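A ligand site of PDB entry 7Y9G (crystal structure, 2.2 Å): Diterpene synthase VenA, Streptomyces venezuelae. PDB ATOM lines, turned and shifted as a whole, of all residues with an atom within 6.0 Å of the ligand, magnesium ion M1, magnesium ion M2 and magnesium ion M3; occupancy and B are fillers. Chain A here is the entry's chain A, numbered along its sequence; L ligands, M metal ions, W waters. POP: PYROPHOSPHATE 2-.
The side-chain hydroxyl (OH) of Tyr 336 lies within hydrogen-bond range of an oxygen (O5) of the ligand (2.5 Å). NE of Arg 335 is in salt-bridge range of O5 of the ligand, 2.7 Å away. NH1 of Arg 202 lies within salt-bridge range of O1 of the ligand, 2.7 Å away. An oxygen (O6) of the ligand lies close to the side-chain amino group (NZ) of Lys 254, 2.9 Å away.
O of Glu 255 sits at hydrogen-bond distance from N of Asp 260 (3.2 Å). OH of Tyr 336 is in hydrogen-bond range of ND2 of Asn 247, at 2.9 Å. The side-chain amide oxygen (OD1) of Asn 247 sits close to the guanidinium group (NH2) of Arg 202. NH2 of Arg 335 sits at hydrogen-bond distance from OG of Ser 107 (2.8 Å). OD1 of Asp 248 is in salt-bridge range of NH2 of Arg 202 (2.9 Å). The guanidinium group (NE) of Arg 202 sits at hydrogen-bond distance from the backbone carbonyl oxygen (O) of Met 262, 3.4 Å away. The side-chain amide oxygen (OE1) of Gln 258 sits at hydrogen-bond distance from the side-chain amino group (NZ) of Lys 254 (3.2 Å). OE1 of Glu 183 lies within hydrogen-bond range of OG of Ser 205, 2.7 Å away.
CD1 of Phe 206 touches O1 of the ligand (3.5 Å). The nearest printed residue that does not touch the ligand is Asp 248 (5.1 Å).
Residues that only touch magnesium ion M1: Lys 254 (3.7 Å). Within 4 Å of magnesium ion M1: Asp 106 and Lys 254. The nearest printed residue that does not touch magnesium ion M1 is Arg 335 (4.2 Å).
Residues that only touch magnesium ion M2: Glu 183 (3.6 Å). Two residues have an atom within 4 Å of magnesium ion M2: Asp 106 and Glu 183.
Three residues have an atom within 4 Å of magnesium ion M3: Asn 247, Ser 251 and Glu 255.
Magnesium ion M1 is bound by O3 of the ligand (2.1 Å), OD2 of Asp 106 (2.1 Å), water W7 (2.1 Å), water W2 (2.1 Å), O6 of the ligand (2.1 Å) and water W3 (2.1 Å). Magnesium ion M1 has six donor atoms within binding distance.
Magnesium ion M2 is bound by water W8, water W9, the side-chain carboxylate of Asp 106, an oxygen (O3) of the ligand, water W2 and water W5. Magnesium ion M2 has six donor atoms within binding distance.
Magnesium ion M3 is bound by OE2 of Glu 255 (2.1 Å), OD1 of Asn 247 (2.1 Å), O2 of the ligand (2.1 Å), water W10 (2.1 Å), O4 of the ligand (2.1 Å) and OG of Ser 251 (2.2 Å). Magnesium ion M3 has six donor atoms within binding distance.
Water W7 lies within hydrogen-bond range of the side-chain carboxylate (OD2) of Asp 260 (3.0 Å) and the side-chain amino group (NZ) of Lys 254 (3.4 Å). Water W3 bridges OG of Ser 110 (2.8 Å) and NZ of Lys 254 (3.0 Å). Water W5 bridges O of Ser 205 and O1 of the ligand. Water W9 bridges the side-chain carboxylate (OE1) of Glu 183 (2.4 Å) and the guanidinium group (NH1) of Arg 202 (3.2 Å). Water W8 lies within hydrogen-bond range of OE2 of Glu 183 (2.4 Å) and SG of Cys 180 (3.5 Å). Water W4 bridges O of Met 262 and NH1 of Arg 202.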
ATOM      1  N   THR A 103     -22.005   1.577 -18.977  1.00  0.00           N
ATOM      2  CA  THR A 103     -21.021   2.662 -18.967  1.00  0.00           C
ATOM      3  C   THR A 103     -21.421   3.674 -20.041  1.00  0.00           C
ATOM      4  O   THR A 103     -21.296   4.875 -19.779  1.00  0.00           O
ATOM      5  CB  THR A 103     -19.589   2.153 -19.137  1.00  0.00           C
ATOM      6  OG1 THR A 103     -19.301   1.236 -18.079  1.00  0.00           O
ATOM      7  CG2 THR A 103     -18.592   3.281 -19.072  1.00  0.00           C
ATOM      8  N   ASP A 106     -24.237   5.399 -18.330  1.00  0.00           N
ATOM      9  CA  ASP A 106     -23.682   6.244 -17.244  1.00  0.00           C
ATOM     10  C   ASP A 106     -23.134   7.536 -17.826  1.00  0.00           C
ATOM     11  O   ASP A 106     -23.347   8.577 -17.199  1.00  0.00           O
ATOM     12  CB  ASP A 106     -22.542   5.586 -16.481  1.00  0.00           C
ATOM     13  CG  ASP A 106     -22.161   6.404 -15.252  1.00  0.00           C
ATOM     14  OD1 ASP A 106     -22.979   6.429 -14.325  1.00  0.00           O
ATOM     15  OD2 ASP A 106     -21.066   7.050 -15.257  1.00  0.00           O
ATOM     16  N   SER A 107     -22.414   7.443 -18.958  1.00  0.00           N
ATOM     17  CA  SER A 107     -21.754   8.591 -19.629  1.00  0.00           C
ATOM     18  C   SER A 107     -22.805   9.510 -20.269  1.00  0.00           C
ATOM     19  O   SER A 107     -22.610  10.713 -20.187  1.00  0.00           O
ATOM     20  CB  SER A 107     -20.734   8.141 -20.654  1.00  0.00           C
ATOM     21  OG  SER A 107     -19.670   7.462 -20.009  1.00  0.00           O
ATOM     22  N   SER A 110     -25.017  11.344 -17.270  1.00  0.00           N
ATOM     23  CA  SER A 110     -24.143  12.232 -16.454  1.00  0.00           C
ATOM     24  C   SER A 110     -23.651  13.393 -17.317  1.00  0.00           C
ATOM     25  O   SER A 110     -22.947  14.271 -16.777  1.00  0.00           O
ATOM     26  CB  SER A 110     -22.993  11.459 -15.852  1.00  0.00           C
ATOM     27  OG  SER A 110     -21.780  11.691 -16.560  1.00  0.00           O
ATOM     28  N   PHE A 176     -30.722   1.229 -10.364  1.00  0.00           N
ATOM     29  CA  PHE A 176     -29.687   1.992 -11.118  1.00  0.00           C
ATOM     30  C   PHE A 176     -30.308   3.304 -11.601  1.00  0.00           C
ATOM     31  O   PHE A 176     -29.713   4.386 -11.354  1.00  0.00           O
ATOM     32  CB  PHE A 176     -29.114   1.144 -12.257  1.00  0.00           C
ATOM     33  CG  PHE A 176     -28.127   1.879 -13.138  1.00  0.00           C
ATOM     34  CD1 PHE A 176     -26.880   2.263 -12.652  1.00  0.00           C
ATOM     35  CD2 PHE A 176     -28.468   2.219 -14.446  1.00  0.00           C
ATOM     36  CE1 PHE A 176     -26.004   2.977 -13.460  1.00  0.00           C
ATOM     37  CE2 PHE A 176     -27.581   2.914 -15.252  1.00  0.00           C
ATOM     38  CZ  PHE A 176     -26.358   3.301 -14.748  1.00  0.00           C
ATOM     39  N   CYS A 180     -29.342   7.141 -10.859  1.00  0.00           N
ATOM     40  CA  CYS A 180     -28.967   8.149 -11.897  1.00  0.00           C
ATOM     41  C   CYS A 180     -29.869   9.380 -11.806  1.00  0.00           C
ATOM     42  O   CYS A 180     -29.371  10.517 -11.940  1.00  0.00           O
ATOM     43  CB  CYS A 180     -29.042   7.545 -13.302  1.00  0.00           C
ATOM     44  SG  CYS A 180     -27.821   6.225 -13.568  1.00  0.00           S
ATOM     45  N   GLU A 183     -28.929  11.659  -8.889  1.00  0.00           N
ATOM     46  CA  GLU A 183     -27.668  12.363  -9.263  1.00  0.00           C
ATOM     47  C   GLU A 183     -28.000  13.510 -10.210  1.00  0.00           C
ATOM     48  O   GLU A 183     -27.487  14.629 -10.029  1.00  0.00           O
ATOM     49  CB  GLU A 183     -26.698  11.423  -9.966  1.00  0.00           C
ATOM     50  CG  GLU A 183     -26.174  10.297  -9.103  1.00  0.00           C
ATOM     51  CD  GLU A 183     -25.250   9.315  -9.821  1.00  0.00           C
ATOM     52  OE1 GLU A 183     -24.400   8.712  -9.141  1.00  0.00           O
ATOM     53  OE2 GLU A 183     -25.369   9.146 -11.076  1.00  0.00           O
ATOM     54  N   ARG A 202     -25.551   6.183  -3.992  1.00  0.00           N
ATOM     55  CA  ARG A 202     -24.574   5.478  -4.866  1.00  0.00           C
ATOM     56  C   ARG A 202     -24.770   3.966  -4.793  1.00  0.00           C
ATOM     57  O   ARG A 202     -24.308   3.292  -5.725  1.00  0.00           O
ATOM     58  CB  ARG A 202     -23.154   5.930  -4.508  1.00  0.00           C
ATOM     59  CG  ARG A 202     -22.855   7.351  -4.919  1.00  0.00           C
ATOM     60  CD  ARG A 202     -22.378   7.355  -6.349  1.00  0.00           C
ATOM     61  NE  ARG A 202     -20.964   7.047  -6.446  1.00  0.00           N
ATOM     62  CZ  ARG A 202     -20.375   6.404  -7.453  1.00  0.00           C
ATOM     63  NH1 ARG A 202     -21.083   5.936  -8.469  1.00  0.00           N
ATOM     64  NH2 ARG A 202     -19.068   6.214  -7.428  1.00  0.00           N
ATOM     65  N   SER A 205     -27.001   3.981  -7.701  1.00  0.00           N
ATOM     66  CA  SER A 205     -26.467   4.590  -8.937  1.00  0.00           C
ATOM     67  C   SER A 205     -25.223   3.815  -9.413  1.00  0.00           C
ATOM     68  O   SER A 205     -24.961   3.810 -10.630  1.00  0.00           O
ATOM     69  CB  SER A 205     -26.250   6.064  -8.778  1.00  0.00           C
ATOM     70  OG  SER A 205     -25.067   6.378  -8.062  1.00  0.00           O
ATOM     71  N   PHE A 206     -24.497   3.190  -8.493  1.00  0.00           N
ATOM     72  CA  PHE A 206     -23.288   2.374  -8.767  1.00  0.00           C
ATOM     73  C   PHE A 206     -23.703   1.011  -9.306  1.00  0.00           C
ATOM     74  O   PHE A 206     -22.852   0.299  -9.794  1.00  0.00           O
ATOM     75  CB  PHE A 206     -22.400   2.223  -7.518  1.00  0.00           C
ATOM     76  CG  PHE A 206     -21.018   1.693  -7.781  1.00  0.00           C
ATOM     77  CD1 PHE A 206     -20.036   2.509  -8.319  1.00  0.00           C
ATOM     78  CD2 PHE A 206     -20.691   0.374  -7.489  1.00  0.00           C
ATOM     79  CE1 PHE A 206     -18.766   2.013  -8.575  1.00  0.00           C
ATOM     80  CE2 PHE A 206     -19.423  -0.117  -7.732  1.00  0.00           C
ATOM     81  CZ  PHE A 206     -18.463   0.695  -8.288  1.00  0.00           C
ATOM     82  N   ASN A 247     -13.570   3.972  -6.580  1.00  0.00           N
ATOM     83  CA  ASN A 247     -14.014   4.599  -7.829  1.00  0.00           C
ATOM     84  C   ASN A 247     -13.971   6.121  -7.633  1.00  0.00           C
ATOM     85  O   ASN A 247     -13.520   6.785  -8.537  1.00  0.00           O
ATOM     86  CB  ASN A 247     -15.375   4.092  -8.319  1.00  0.00           C
ATOM     87  CG  ASN A 247     -15.811   4.805  -9.584  1.00  0.00           C
ATOM     88  OD1 ASN A 247     -16.341   5.906  -9.520  1.00  0.00           O
ATOM     89  ND2 ASN A 247     -15.513   4.217 -10.728  1.00  0.00           N
ATOM     90  N   ASP A 248     -14.441   6.665  -6.516  1.00  0.00           N
ATOM     91  CA  ASP A 248     -14.454   8.144  -6.320  1.00  0.00           C
ATOM     92  C   ASP A 248     -13.028   8.684  -6.421  1.00  0.00           C
ATOM     93  O   ASP A 248     -12.838   9.729  -7.076  1.00  0.00           O
ATOM     94  CB  ASP A 248     -15.127   8.535  -5.010  1.00  0.00           C
ATOM     95  CG  ASP A 248     -16.620   8.325  -5.028  1.00  0.00           C
ATOM     96  OD1 ASP A 248     -17.139   7.927  -6.079  1.00  0.00           O
ATOM     97  OD2 ASP A 248     -17.251   8.479  -3.951  1.00  0.00           O
ATOM     98  N   SER A 251     -11.694   8.105 -10.152  1.00  0.00           N
ATOM     99  CA  SER A 251     -12.558   8.827 -11.124  1.00  0.00           C
ATOM    100  C   SER A 251     -12.604  10.333 -10.813  1.00  0.00           C
ATOM    101  O   SER A 251     -13.205  11.054 -11.612  1.00  0.00           O
ATOM    102  CB  SER A 251     -13.937   8.184 -11.243  1.00  0.00           C
ATOM    103  OG  SER A 251     -14.767   8.389 -10.110  1.00  0.00           O
ATOM    104  N   TRP A 252     -11.935  10.833  -9.754  1.00  0.00           N
ATOM    105  CA  TRP A 252     -12.047  12.278  -9.393  1.00  0.00           C
ATOM    106  C   TRP A 252     -11.513  13.180 -10.518  1.00  0.00           C
ATOM    107  O   TRP A 252     -12.154  14.201 -10.802  1.00  0.00           O
ATOM    108  CB  TRP A 252     -11.359  12.588  -8.045  1.00  0.00           C
ATOM    109  CG  TRP A 252     -11.345  14.053  -7.709  1.00  0.00           C
ATOM    110  CD1 TRP A 252     -10.241  14.824  -7.499  1.00  0.00           C
ATOM    111  CD2 TRP A 252     -12.469  14.948  -7.580  1.00  0.00           C
ATOM    112  NE1 TRP A 252     -10.604  16.116  -7.205  1.00  0.00           N
ATOM    113  CE2 TRP A 252     -11.960  16.228  -7.277  1.00  0.00           C
ATOM    114  CE3 TRP A 252     -13.861  14.794  -7.680  1.00  0.00           C
ATOM    115  CZ2 TRP A 252     -12.784  17.334  -7.042  1.00  0.00           C
ATOM    116  CZ3 TRP A 252     -14.680  15.890  -7.471  1.00  0.00           C
ATOM    117  CH2 TRP A 252     -14.145  17.144  -7.161  1.00  0.00           C
ATOM    118  N   LYS A 254     -11.725  13.012 -13.563  1.00  0.00           N
ATOM    119  CA  LYS A 254     -12.716  13.178 -14.651  1.00  0.00           C
ATOM    120  C   LYS A 254     -13.985  13.822 -14.084  1.00  0.00           C
ATOM    121  O   LYS A 254     -14.599  14.615 -14.790  1.00  0.00           O
ATOM    122  CB  LYS A 254     -12.963  11.845 -15.373  1.00  0.00           C
ATOM    123  CG  LYS A 254     -14.218  11.067 -15.016  1.00  0.00           C
ATOM    124  CD  LYS A 254     -14.906  10.426 -16.217  1.00  0.00           C
ATOM    125  CE  LYS A 254     -15.960   9.396 -15.854  1.00  0.00           C
ATOM    126  NZ  LYS A 254     -17.196  10.019 -15.335  1.00  0.00           N
ATOM    127  N   GLU A 255     -14.373  13.524 -12.842  1.00  0.00           N
ATOM    128  CA  GLU A 255     -15.635  14.054 -12.262  1.00  0.00           C
ATOM    129  C   GLU A 255     -15.435  15.538 -11.911  1.00  0.00           C
ATOM    130  O   GLU A 255     -16.396  16.306 -12.029  1.00  0.00           O
ATOM    131  CB  GLU A 255     -16.077  13.134 -11.122  1.00  0.00           C
ATOM    132  CG  GLU A 255     -16.561  11.809 -11.664  1.00  0.00           C
ATOM    133  CD  GLU A 255     -16.877  10.757 -10.622  1.00  0.00           C
ATOM    134  OE1 GLU A 255     -16.753  11.073  -9.437  1.00  0.00           O
ATOM    135  OE2 GLU A 255     -17.219   9.622 -11.014  1.00  0.00           O
ATOM    136  N   GLN A 258     -15.990  17.251 -15.148  1.00  0.00           N
ATOM    137  CA  GLN A 258     -17.408  17.072 -15.587  1.00  0.00           C
ATOM    138  C   GLN A 258     -18.410  17.650 -14.577  1.00  0.00           C
ATOM    139  O   GLN A 258     -19.618  17.564 -14.840  1.00  0.00           O
ATOM    140  CB  GLN A 258     -17.659  15.587 -15.839  1.00  0.00           C
ATOM    141  CG  GLN A 258     -16.932  15.048 -17.062  1.00  0.00           C
ATOM    142  CD  GLN A 258     -17.122  13.561 -17.265  1.00  0.00           C
ATOM    143  OE1 GLN A 258     -17.917  12.915 -16.584  1.00  0.00           O
ATOM    144  NE2 GLN A 258     -16.351  12.993 -18.171  1.00  0.00           N
ATOM    145  N   ASP A 260     -19.579  16.685 -11.742  1.00  0.00           N
ATOM    146  CA  ASP A 260     -20.417  15.671 -11.037  1.00  0.00           C
ATOM    147  C   ASP A 260     -20.365  15.940  -9.524  1.00  0.00           C
ATOM    148  O   ASP A 260     -19.293  16.309  -9.000  1.00  0.00           O
ATOM    149  CB  ASP A 260     -19.955  14.245 -11.325  1.00  0.00           C
ATOM    150  CG  ASP A 260     -20.241  13.808 -12.751  1.00  0.00           C
ATOM    151  OD1 ASP A 260     -21.221  14.342 -13.357  1.00  0.00           O
ATOM    152  OD2 ASP A 260     -19.489  12.965 -13.258  1.00  0.00           O
ATOM    153  N   MET A 262     -22.005  13.673  -7.161  1.00  0.00           N
ATOM    154  CA  MET A 262     -22.227  12.411  -6.399  1.00  0.00           C
ATOM    155  C   MET A 262     -20.906  11.638  -6.274  1.00  0.00           C
ATOM    156  O   MET A 262     -20.803  10.464  -6.724  1.00  0.00           O
ATOM    157  CB  MET A 262     -23.338  11.591  -7.058  1.00  0.00           C
ATOM    158  CG  MET A 262     -24.043  10.672  -6.092  1.00  0.00           C
ATOM    159  SD  MET A 262     -24.958  11.530  -4.768  1.00  0.00           S
ATOM    160  CE  MET A 262     -26.131  12.518  -5.692  1.00  0.00           C
ATOM    161  N   ARG A 335     -10.607   6.184 -19.342  1.00  0.00           N
ATOM    162  CA  ARG A 335     -11.813   6.875 -18.829  1.00  0.00           C
ATOM    163  C   ARG A 335     -11.390   7.834 -17.692  1.00  0.00           C
ATOM    164  O   ARG A 335     -12.009   8.874 -17.551  1.00  0.00           O
ATOM    165  CB  ARG A 335     -12.834   5.836 -18.358  1.00  0.00           C
ATOM    166  CG  ARG A 335     -14.182   6.382 -17.935  1.00  0.00           C
ATOM    167  CD  ARG A 335     -15.140   5.271 -17.526  1.00  0.00           C
ATOM    168  NE  ARG A 335     -16.436   5.787 -17.084  1.00  0.00           N
ATOM    169  CZ  ARG A 335     -17.354   6.337 -17.884  1.00  0.00           C
ATOM    170  NH1 ARG A 335     -18.493   6.767 -17.368  1.00  0.00           N
ATOM    171  NH2 ARG A 335     -17.144   6.435 -19.194  1.00  0.00           N
ATOM    172  N   TYR A 336     -10.371   7.491 -16.900  1.00  0.00           N
ATOM    173  CA  TYR A 336      -9.950   8.257 -15.698  1.00  0.00           C
ATOM    174  C   TYR A 336      -8.631   8.992 -15.968  1.00  0.00           C
ATOM    175  O   TYR A 336      -8.452  10.137 -15.499  1.00  0.00           O
ATOM    176  CB  TYR A 336      -9.879   7.332 -14.481  1.00  0.00           C
ATOM    177  CG  TYR A 336     -11.167   6.585 -14.202  1.00  0.00           C
ATOM    178  CD1 TYR A 336     -12.409   7.121 -14.515  1.00  0.00           C
ATOM    179  CD2 TYR A 336     -11.139   5.332 -13.640  1.00  0.00           C
ATOM    180  CE1 TYR A 336     -13.586   6.420 -14.259  1.00  0.00           C
ATOM    181  CE2 TYR A 336     -12.299   4.620 -13.392  1.00  0.00           C
ATOM    182  CZ  TYR A 336     -13.532   5.160 -13.705  1.00  0.00           C
ATOM    183  OH  TYR A 336     -14.653   4.419 -13.455  1.00  0.00           O
HETATM  184  P1  POP L   1     -19.564   6.201 -11.587  1.00  0.00           P
HETATM  185  O1  POP L   1     -20.031   5.030 -10.777  1.00  0.00           O
HETATM  186  O2  POP L   1     -18.747   7.203 -10.815  1.00  0.00           O
HETATM  187  O3  POP L   1     -20.646   6.934 -12.415  1.00  0.00           O
HETATM  188  O   POP L   1     -18.462   5.543 -12.650  1.00  0.00           O
HETATM  189  P2  POP L   1     -17.393   6.443 -13.473  1.00  0.00           P
HETATM  190  O4  POP L   1     -16.438   6.909 -12.377  1.00  0.00           O
HETATM  191  O5  POP L   1     -16.707   5.534 -14.433  1.00  0.00           O
HETATM  192  O6  POP L   1     -18.228   7.550 -14.104  1.00  0.00           O
HETATM  193 MG    MG M   1     -20.166   8.327 -13.879  1.00  0.00          MG
HETATM  194 MG    MG M   2     -22.711   7.026 -12.373  1.00  0.00          MG
HETATM  195 MG    MG M   3     -16.771   7.690 -10.463  1.00  0.00          MG
HETATM  196  O   HOH W   1     -18.963   2.382 -11.874  1.00  0.00           O
HETATM  197  O   HOH W   2     -22.141   8.771 -13.337  1.00  0.00           O
HETATM  198  O   HOH W   3     -20.200   9.653 -15.533  1.00  0.00           O
HETATM  199  O   HOH W   4     -20.413   9.232  -9.154  1.00  0.00           O
HETATM  200  O   HOH W   5     -22.734   4.900 -11.696  1.00  0.00           O
HETATM  201  O   HOH W   6     -18.974   3.142 -15.313  1.00  0.00           O
HETATM  202  O   HOH W   7     -19.428   9.961 -12.817  1.00  0.00           O
HETATM  203  O   HOH W   8     -24.686   7.146 -12.289  1.00  0.00           O
HETATM  204  O   HOH W   9     -22.578   7.874 -10.508  1.00  0.00           O
HETATM  205  O   HOH W  10     -17.190   8.670  -8.677  1.00  0.00           O
